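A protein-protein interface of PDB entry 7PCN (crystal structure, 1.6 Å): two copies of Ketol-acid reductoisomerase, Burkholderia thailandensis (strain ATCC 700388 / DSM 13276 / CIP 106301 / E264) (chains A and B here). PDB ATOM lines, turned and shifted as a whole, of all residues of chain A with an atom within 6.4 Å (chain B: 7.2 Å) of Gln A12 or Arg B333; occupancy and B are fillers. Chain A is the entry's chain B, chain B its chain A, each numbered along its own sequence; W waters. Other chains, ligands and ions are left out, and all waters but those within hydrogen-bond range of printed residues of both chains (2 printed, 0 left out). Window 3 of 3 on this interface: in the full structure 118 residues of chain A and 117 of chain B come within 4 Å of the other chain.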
ATOM      1  N   ILE A  10     -13.451  22.409   8.610  1.00  0.00           N
ATOM      2  CA  ILE A  10     -12.336  23.048   9.357  1.00  0.00           C
ATOM      3  C   ILE A  10     -12.424  22.577  10.804  1.00  0.00           C
ATOM      4  O   ILE A  10     -13.459  22.776  11.424  1.00  0.00           O
ATOM      5  CB  ILE A  10     -12.371  24.582   9.241  1.00  0.00           C
ATOM      6  CG1 ILE A  10     -12.305  25.018   7.775  1.00  0.00           C
ATOM      7  CG2 ILE A  10     -11.238  25.179  10.052  1.00  0.00           C
ATOM      8  CD1 ILE A  10     -12.678  26.459   7.539  1.00  0.00           C
ATOM      9  N   TYR A  11     -11.348  21.980  11.289  1.00  0.00           N
ATOM     10  CA  TYR A  11     -11.245  21.356  12.627  1.00  0.00           C
ATOM     11  C   TYR A  11     -10.388  22.253  13.516  1.00  0.00           C
ATOM     12  O   TYR A  11      -9.227  22.569  13.145  1.00  0.00           O
ATOM     13  CB  TYR A  11     -10.623  19.962  12.515  1.00  0.00           C
ATOM     14  CG  TYR A  11     -11.484  18.914  11.854  1.00  0.00           C
ATOM     15  CD1 TYR A  11     -11.637  18.849  10.477  1.00  0.00           C
ATOM     16  CD2 TYR A  11     -12.119  17.957  12.619  1.00  0.00           C
ATOM     17  CE1 TYR A  11     -12.441  17.886   9.882  1.00  0.00           C
ATOM     18  CE2 TYR A  11     -12.910  16.974  12.048  1.00  0.00           C
ATOM     19  CZ  TYR A  11     -13.066  16.931  10.673  1.00  0.00           C
ATOM     20  OH  TYR A  11     -13.860  15.966  10.129  1.00  0.00           O
ATOM     21  N   GLN A  12     -10.941  22.640  14.662  1.00  0.00           N
ATOM     22  CA  GLN A  12     -10.199  23.357  15.726  1.00  0.00           C
ATOM     23  C   GLN A  12     -10.090  22.405  16.925  1.00  0.00           C
ATOM     24  O   GLN A  12     -10.420  21.216  16.757  1.00  0.00           O
ATOM     25  CB  GLN A  12     -10.880  24.707  15.959  1.00  0.00           C
ATOM     26  CG  GLN A  12     -10.799  25.601  14.727  1.00  0.00           C
ATOM     27  CD  GLN A  12     -11.357  26.989  14.934  1.00  0.00           C
ATOM     28  OE1 GLN A  12     -12.029  27.285  15.921  1.00  0.00           O
ATOM     29  NE2 GLN A  12     -11.062  27.870  13.995  1.00  0.00           N
ATOM     30  N   ASP A  13      -9.592  22.873  18.070  1.00  0.00           N
ATOM     31  CA  ASP A  13      -9.307  22.003  19.246  1.00  0.00           C
ATOM     32  C   ASP A  13     -10.570  21.247  19.685  1.00  0.00           C
ATOM     33  O   ASP A  13     -10.417  20.083  20.131  1.00  0.00           O
ATOM     34  CB  ASP A  13      -8.774  22.802  20.432  1.00  0.00           C
ATOM     35  CG  ASP A  13      -7.275  23.083  20.438  1.00  0.00           C
ATOM     36  OD1 ASP A  13      -6.527  22.539  19.572  1.00  0.00           O
ATOM     37  OD2 ASP A  13      -6.865  23.852  21.317  1.00  0.00           O
ATOM     38  N   GLU A  14     -11.749  21.887  19.603  1.00  0.00           N
ATOM     39  CA  GLU A  14     -13.067  21.312  20.006  1.00  0.00           C
ATOM     40  C   GLU A  14     -13.389  20.077  19.150  1.00  0.00           C
ATOM     41  O   GLU A  14     -14.284  19.322  19.552  1.00  0.00           O
ATOM     42  CB  GLU A  14     -14.259  22.259  19.811  1.00  0.00           C
ATOM     43  CG  GLU A  14     -14.119  23.635  20.412  1.00  0.00           C
ATOM     44  CD  GLU A  14     -13.492  24.611  19.434  1.00  0.00           C
ATOM     45  OE1 GLU A  14     -12.286  24.791  19.535  1.00  0.00           O
ATOM     46  OE2 GLU A  14     -14.212  25.137  18.539  1.00  0.00           O
ATOM     47  N   HIS A  15     -12.719  19.893  18.005  1.00  0.00           N
ATOM     48  CA  HIS A  15     -13.057  18.851  17.003  1.00  0.00           C
ATOM     49  C   HIS A  15     -11.981  17.759  16.941  1.00  0.00           C
ATOM     50  O   HIS A  15     -12.047  16.940  16.020  1.00  0.00           O
ATOM     51  CB  HIS A  15     -13.270  19.476  15.623  1.00  0.00           C
ATOM     52  CG  HIS A  15     -14.203  20.634  15.616  1.00  0.00           C
ATOM     53  ND1 HIS A  15     -13.750  21.936  15.522  1.00  0.00           N
ATOM     54  CD2 HIS A  15     -15.553  20.695  15.674  1.00  0.00           C
ATOM     55  CE1 HIS A  15     -14.781  22.756  15.532  1.00  0.00           C
ATOM     56  NE2 HIS A  15     -15.905  22.016  15.627  1.00  0.00           N
ATOM     57  N   ALA A  16     -11.047  17.726  17.894  1.00  0.00           N
ATOM     58  CA  ALA A  16      -9.912  16.780  17.878  1.00  0.00           C
ATOM     59  C   ALA A  16      -9.511  16.477  19.315  1.00  0.00           C
ATOM     60  O   ALA A  16      -9.876  17.240  20.229  1.00  0.00           O
ATOM     61  CB  ALA A  16      -8.765  17.336  17.073  1.00  0.00           C
ATOM     62  N   GLY A 149       0.955  28.843  23.311  1.00  0.00           N
ATOM     63  CA  GLY A 149      -0.416  28.293  23.330  1.00  0.00           C
ATOM     64  C   GLY A 149      -1.181  28.658  22.067  1.00  0.00           C
ATOM     65  O   GLY A 149      -2.433  28.671  22.110  1.00  0.00           O
ATOM     66  N   GLY A 151      -1.118  28.410  17.387  1.00  0.00           N
ATOM     67  CA  GLY A 151      -0.838  27.464  16.299  1.00  0.00           C
ATOM     68  C   GLY A 151      -0.960  28.154  14.961  1.00  0.00           C
ATOM     69  O   GLY A 151      -1.470  29.292  14.927  1.00  0.00           O
ATOM     70  N   ALA A 152      -0.493  27.487  13.913  1.00  0.00           N
ATOM     71  CA  ALA A 152      -0.633  27.925  12.513  1.00  0.00           C
ATOM     72  C   ALA A 152      -1.597  26.968  11.827  1.00  0.00           C
ATOM     73  O   ALA A 152      -1.786  25.842  12.285  1.00  0.00           O
ATOM     74  CB  ALA A 152       0.709  27.936  11.827  1.00  0.00           C
ATOM     75  N   PRO A 153      -2.234  27.388  10.719  1.00  0.00           N
ATOM     76  CA  PRO A 153      -3.166  26.527  10.001  1.00  0.00           C
ATOM     77  C   PRO A 153      -2.447  25.348   9.333  1.00  0.00           C
ATOM     78  O   PRO A 153      -1.242  25.391   9.155  1.00  0.00           O
ATOM     79  CB  PRO A 153      -3.780  27.416   8.910  1.00  0.00           C
ATOM     80  CG  PRO A 153      -3.429  28.834   9.329  1.00  0.00           C
ATOM     81  CD  PRO A 153      -2.132  28.724  10.115  1.00  0.00           C
ATOM     82  N   ARG A 175      -3.572  18.207  16.598  1.00  0.00           N
ATOM     83  CA  ARG A 175      -3.826  18.869  17.905  1.00  0.00           C
ATOM     84  C   ARG A 175      -2.544  18.879  18.743  1.00  0.00           C
ATOM     85  O   ARG A 175      -2.277  19.904  19.387  1.00  0.00           O
ATOM     86  CB  ARG A 175      -4.969  18.193  18.657  1.00  0.00           C
ATOM     87  CG  ARG A 175      -5.222  18.790  20.025  1.00  0.00           C
ATOM     88  CD  ARG A 175      -6.492  18.297  20.655  1.00  0.00           C
ATOM     89  NE  ARG A 175      -6.474  18.794  22.023  1.00  0.00           N
ATOM     90  CZ  ARG A 175      -7.526  19.226  22.693  1.00  0.00           C
ATOM     91  NH1 ARG A 175      -8.725  19.225  22.133  1.00  0.00           N
ATOM     92  NH2 ARG A 175      -7.365  19.668  23.925  1.00  0.00           N
ATOM     93  N   PHE A 179      -1.792  22.715  15.369  1.00  0.00           N
ATOM     94  CA  PHE A 179      -2.433  23.299  14.155  1.00  0.00           C
ATOM     95  C   PHE A 179      -3.932  23.536  14.380  1.00  0.00           C
ATOM     96  O   PHE A 179      -4.481  24.493  13.776  1.00  0.00           O
ATOM     97  CB  PHE A 179      -2.222  22.435  12.914  1.00  0.00           C
ATOM     98  CG  PHE A 179      -0.774  22.135  12.633  1.00  0.00           C
ATOM     99  CD1 PHE A 179       0.138  23.153  12.386  1.00  0.00           C
ATOM    100  CD2 PHE A 179      -0.324  20.828  12.627  1.00  0.00           C
ATOM    101  CE1 PHE A 179       1.473  22.869  12.150  1.00  0.00           C
ATOM    102  CE2 PHE A 179       1.006  20.544  12.389  1.00  0.00           C
ATOM    103  CZ  PHE A 179       1.899  21.559  12.130  1.00  0.00           C
ATOM    104  N   THR A 180      -4.585  22.709  15.202  1.00  0.00           N
ATOM    105  CA  THR A 180      -6.034  22.851  15.507  1.00  0.00           C
ATOM    106  C   THR A 180      -6.284  24.145  16.304  1.00  0.00           C
ATOM    107  O   THR A 180      -7.443  24.582  16.385  1.00  0.00           O
ATOM    108  CB  THR A 180      -6.599  21.591  16.176  1.00  0.00           C
ATOM    109  OG1 THR A 180      -5.835  21.270  17.338  1.00  0.00           O
ATOM    110  CG2 THR A 180      -6.617  20.416  15.220  1.00  0.00           C
ATOM    111  N   ARG A 181      -5.255  24.769  16.873  1.00  0.00           N
ATOM    112  CA  ARG A 181      -5.459  26.057  17.592  1.00  0.00           C
ATOM    113  C   ARG A 181      -5.774  27.189  16.599  1.00  0.00           C
ATOM    114  O   ARG A 181      -6.332  28.210  17.032  1.00  0.00           O
ATOM    115  CB  ARG A 181      -4.227  26.409  18.416  1.00  0.00           C
ATOM    116  CG  ARG A 181      -3.882  25.366  19.463  1.00  0.00           C
ATOM    117  CD  ARG A 181      -2.479  25.595  19.971  1.00  0.00           C
ATOM    118  NE  ARG A 181      -2.140  24.601  20.976  1.00  0.00           N
ATOM    119  CZ  ARG A 181      -1.017  24.585  21.677  1.00  0.00           C
ATOM    120  NH1 ARG A 181      -0.093  25.505  21.472  1.00  0.00           N
ATOM    121  NH2 ARG A 181      -0.816  23.637  22.570  1.00  0.00           N
ATOM    122  N   ALA A 182      -5.412  27.021  15.328  1.00  0.00           N
ATOM    123  CA  ALA A 182      -5.748  27.944  14.223  1.00  0.00           C
ATOM    124  C   ALA A 182      -6.899  27.347  13.416  1.00  0.00           C
ATOM    125  O   ALA A 182      -7.970  27.977  13.306  1.00  0.00           O
ATOM    126  CB  ALA A 182      -4.536  28.176  13.366  1.00  0.00           C
ATOM    127  N   GLY A 183      -6.687  26.141  12.900  1.00  0.00           N
ATOM    128  CA  GLY A 183      -7.694  25.436  12.099  1.00  0.00           C
ATOM    129  C   GLY A 183      -7.047  24.503  11.107  1.00  0.00           C
ATOM    130  O   GLY A 183      -6.056  24.905  10.450  1.00  0.00           O
ATOM    131  N   VAL A 184      -7.604  23.303  10.976  1.00  0.00           N
ATOM    132  CA  VAL A 184      -7.091  22.275  10.032  1.00  0.00           C
ATOM    133  C   VAL A 184      -8.206  22.003   9.025  1.00  0.00           C
ATOM    134  O   VAL A 184      -9.279  21.549   9.430  1.00  0.00           O
ATOM    135  CB  VAL A 184      -6.607  21.026  10.784  1.00  0.00           C
ATOM    136  CG1 VAL A 184      -6.137  19.932   9.832  1.00  0.00           C
ATOM    137  CG2 VAL A 184      -5.501  21.411  11.761  1.00  0.00           C
ATOM    138  N   VAL B 328     -12.217  33.887   5.862  1.00  0.00           N
ATOM    139  CA  VAL B 328     -11.070  33.123   6.426  1.00  0.00           C
ATOM    140  C   VAL B 328     -10.927  33.456   7.918  1.00  0.00           C
ATOM    141  O   VAL B 328     -10.764  32.527   8.738  1.00  0.00           O
ATOM    142  CB  VAL B 328      -9.784  33.398   5.632  1.00  0.00           C
ATOM    143  CG1 VAL B 328      -8.560  32.913   6.379  1.00  0.00           C
ATOM    144  CG2 VAL B 328      -9.859  32.778   4.239  1.00  0.00           C
ATOM    145  N   ARG B 329     -10.994  34.734   8.274  1.00  0.00           N
ATOM    146  CA  ARG B 329     -10.697  35.167   9.661  1.00  0.00           C
ATOM    147  C   ARG B 329     -11.796  34.664  10.610  1.00  0.00           C
ATOM    148  O   ARG B 329     -11.469  34.462  11.797  1.00  0.00           O
ATOM    149  CB  ARG B 329     -10.477  36.683   9.743  1.00  0.00           C
ATOM    150  CG  ARG B 329      -9.736  37.125  11.000  1.00  0.00           C
ATOM    151  CD  ARG B 329      -8.541  36.253  11.385  1.00  0.00           C
ATOM    152  NE  ARG B 329      -7.622  36.149  10.269  1.00  0.00           N
ATOM    153  CZ  ARG B 329      -6.983  35.049   9.850  1.00  0.00           C
ATOM    154  NH1 ARG B 329      -7.115  33.882  10.473  1.00  0.00           N
ATOM    155  NH2 ARG B 329      -6.190  35.147   8.788  1.00  0.00           N
ATOM    156  N   ALA B 330     -13.030  34.448  10.124  1.00  0.00           N
ATOM    157  CA  ALA B 330     -14.148  33.885  10.925  1.00  0.00           C
ATOM    158  C   ALA B 330     -13.959  32.376  11.119  1.00  0.00           C
ATOM    159  O   ALA B 330     -14.517  31.846  12.099  1.00  0.00           O
ATOM    160  CB  ALA B 330     -15.473  34.167  10.264  1.00  0.00           C
ATOM    161  N   ALA B 331     -13.233  31.703  10.218  1.00  0.00           N
ATOM    162  CA  ALA B 331     -13.080  30.226  10.205  1.00  0.00           C
ATOM    163  C   ALA B 331     -11.740  29.758  10.816  1.00  0.00           C
ATOM    164  O   ALA B 331     -11.634  28.576  11.219  1.00  0.00           O
ATOM    165  CB  ALA B 331     -13.235  29.743   8.785  1.00  0.00           C
ATOM    166  N   PHE B 332     -10.724  30.616  10.841  1.00  0.00           N
ATOM    167  CA  PHE B 332      -9.369  30.283  11.347  1.00  0.00           C
ATOM    168  C   PHE B 332      -8.967  31.293  12.419  1.00  0.00           C
ATOM    169  O   PHE B 332      -9.031  32.514  12.202  1.00  0.00           O
ATOM    170  CB  PHE B 332      -8.320  30.318  10.238  1.00  0.00           C
ATOM    171  CG  PHE B 332      -8.467  29.235   9.203  1.00  0.00           C
ATOM    172  CD1 PHE B 332      -9.312  29.410   8.122  1.00  0.00           C
ATOM    173  CD2 PHE B 332      -7.795  28.026   9.327  1.00  0.00           C
ATOM    174  CE1 PHE B 332      -9.434  28.422   7.158  1.00  0.00           C
ATOM    175  CE2 PHE B 332      -7.933  27.033   8.366  1.00  0.00           C
ATOM    176  CZ  PHE B 332      -8.756  27.229   7.287  1.00  0.00           C
ATOM    177  N   ARG B 333      -8.525  30.785  13.557  1.00  0.00           N
ATOM    178  CA  ARG B 333      -8.043  31.647  14.654  1.00  0.00           C
ATOM    179  C   ARG B 333      -6.617  32.091  14.315  1.00  0.00           C
ATOM    180  O   ARG B 333      -5.794  31.238  13.914  1.00  0.00           O
ATOM    181  CB  ARG B 333      -8.146  30.902  15.983  1.00  0.00           C
ATOM    182  CG  ARG B 333      -9.568  30.498  16.357  1.00  0.00           C
ATOM    183  CD  ARG B 333      -9.644  29.548  17.544  1.00  0.00           C
ATOM    184  NE  ARG B 333      -9.573  30.272  18.803  1.00  0.00           N
ATOM    185  CZ  ARG B 333      -8.461  30.754  19.352  1.00  0.00           C
ATOM    186  NH1 ARG B 333      -7.278  30.589  18.778  1.00  0.00           N
ATOM    187  NH2 ARG B 333      -8.533  31.399  20.501  1.00  0.00           N
ATOM    188  N   PHE B 334      -6.341  33.385  14.473  1.00  0.00           N
ATOM    189  CA  PHE B 334      -5.016  33.982  14.194  1.00  0.00           C
ATOM    190  C   PHE B 334      -4.371  34.363  15.521  1.00  0.00           C
ATOM    191  O   PHE B 334      -5.032  34.936  16.379  1.00  0.00           O
ATOM    192  CB  PHE B 334      -5.140  35.180  13.249  1.00  0.00           C
ATOM    193  CG  PHE B 334      -3.806  35.625  12.712  1.00  0.00           C
ATOM    194  CD1 PHE B 334      -3.143  34.884  11.745  1.00  0.00           C
ATOM    195  CD2 PHE B 334      -3.175  36.740  13.243  1.00  0.00           C
ATOM    196  CE1 PHE B 334      -1.889  35.270  11.295  1.00  0.00           C
ATOM    197  CE2 PHE B 334      -1.934  37.132  12.774  1.00  0.00           C
ATOM    198  CZ  PHE B 334      -1.286  36.388  11.815  1.00  0.00           C
ATOM    199  N   PRO B 335      -3.067  34.078  15.741  1.00  0.00           N
ATOM    200  CA  PRO B 335      -2.416  34.453  16.992  1.00  0.00           C
ATOM    201  C   PRO B 335      -2.318  35.979  17.110  1.00  0.00           C
ATOM    202  O   PRO B 335      -1.718  36.606  16.248  1.00  0.00           O
ATOM    203  CB  PRO B 335      -1.010  33.839  16.925  1.00  0.00           C
ATOM    204  CG  PRO B 335      -0.781  33.497  15.465  1.00  0.00           C
ATOM    205  CD  PRO B 335      -2.144  33.419  14.806  1.00  0.00           C
ATOM    206  N   THR B 336      -2.927  36.537  18.151  1.00  0.00           N
ATOM    207  CA  THR B 336      -2.847  37.980  18.471  1.00  0.00           C
ATOM    208  C   THR B 336      -2.456  38.138  19.937  1.00  0.00           C
ATOM    209  O   THR B 336      -2.682  37.201  20.711  1.00  0.00           O
ATOM    210  CB  THR B 336      -4.170  38.691  18.160  1.00  0.00           C
ATOM    211  OG1 THR B 336      -5.173  38.090  18.975  1.00  0.00           O
ATOM    212  CG2 THR B 336      -4.565  38.588  16.704  1.00  0.00           C
HETATM  213  O   HOH W   1      -4.592  30.076  20.849  1.00  0.00           O
HETATM  214  O   HOH W   2     -12.692  30.453  14.287  1.00  0.00           O
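The guanidinium group of Arg B329 sits at hydrogen-bond distance from the backbone carbonyl oxygen of Phe B332 (2.9 Å).
The backbone NH (N) of Gln A12 sits at hydrogen-bond distance from a ring nitrogen (ND1) of His A15, at 3.0 Å.
The side-chain amide nitrogen (NE2) of Gln A12 is in hydrogen-bond range of the backbone carbonyl oxygen (O) of Ala A182 (3.2 Å).
O of Ala B331 is in hydrogen-bond range of NE2 of Gln A12, at 2.9 Å.
O of Arg A181 is in hydrogen-bond range of NH1 of Arg B333.
N of Arg B333 lies within hydrogen-bond range of O of Ala A182 (2.9 Å).
No position is printed for both chains.
Of the 9 pairs that touch across the chains among the printed residues, none has its exchanged pair printed and touching as well.
Of the printed residues of chain B, Ile A10 touches Ala B331 and Phe B332.
Gln A12 touches just these residues of chain B: Ala B331, Phe B332 and Arg B333.
Of the printed residues of chain B, Arg A181 touches Arg B333.
Of the printed residues of chain B, Ala A182 touches Phe B332 and Arg B333.
Of the printed residues of chain A, Ala B331 touches Ile A10 (3.6 Å) and Gln A12 (2.9 Å).
Of the printed residues of chain A, Phe B332 touches Ile A10, Gln A12, Ala A182 and Gly A183.
Arg B333 touches three residues of chain A.
The nearest residue of chain B that does not touch Gln A12 is Ala B330 (5.6 Å).
The nearest printed residue of chain A that does not touch Phe B332 is Pro A153 (4.1 Å).
Of the 9 printed residues of chain B, 3 touch a printed residue of chain A.
Among the printed residues, no Asp or Glu carboxylate lies within 4 Å of a Lys or Arg side-chain nitrogen of the other chain.
Among the printed residues, pairs that only touch across the chains: Ala A182 with Phe B332, Gly A183 with Phe B332, Ile A10 with Ala B331, Gln A12 with Arg B333, Ile A10 with Phe B332 and Gln A12 with Phe B332.
Water W1 lies within hydrogen-bond range of O of Gly A149 (2.9 Å) and NH1 of Arg B333 (3.4 Å).
Water W2 bridges the side-chain amide nitrogen of Gln A12 and the backbone carbonyl oxygen of Ala B330.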
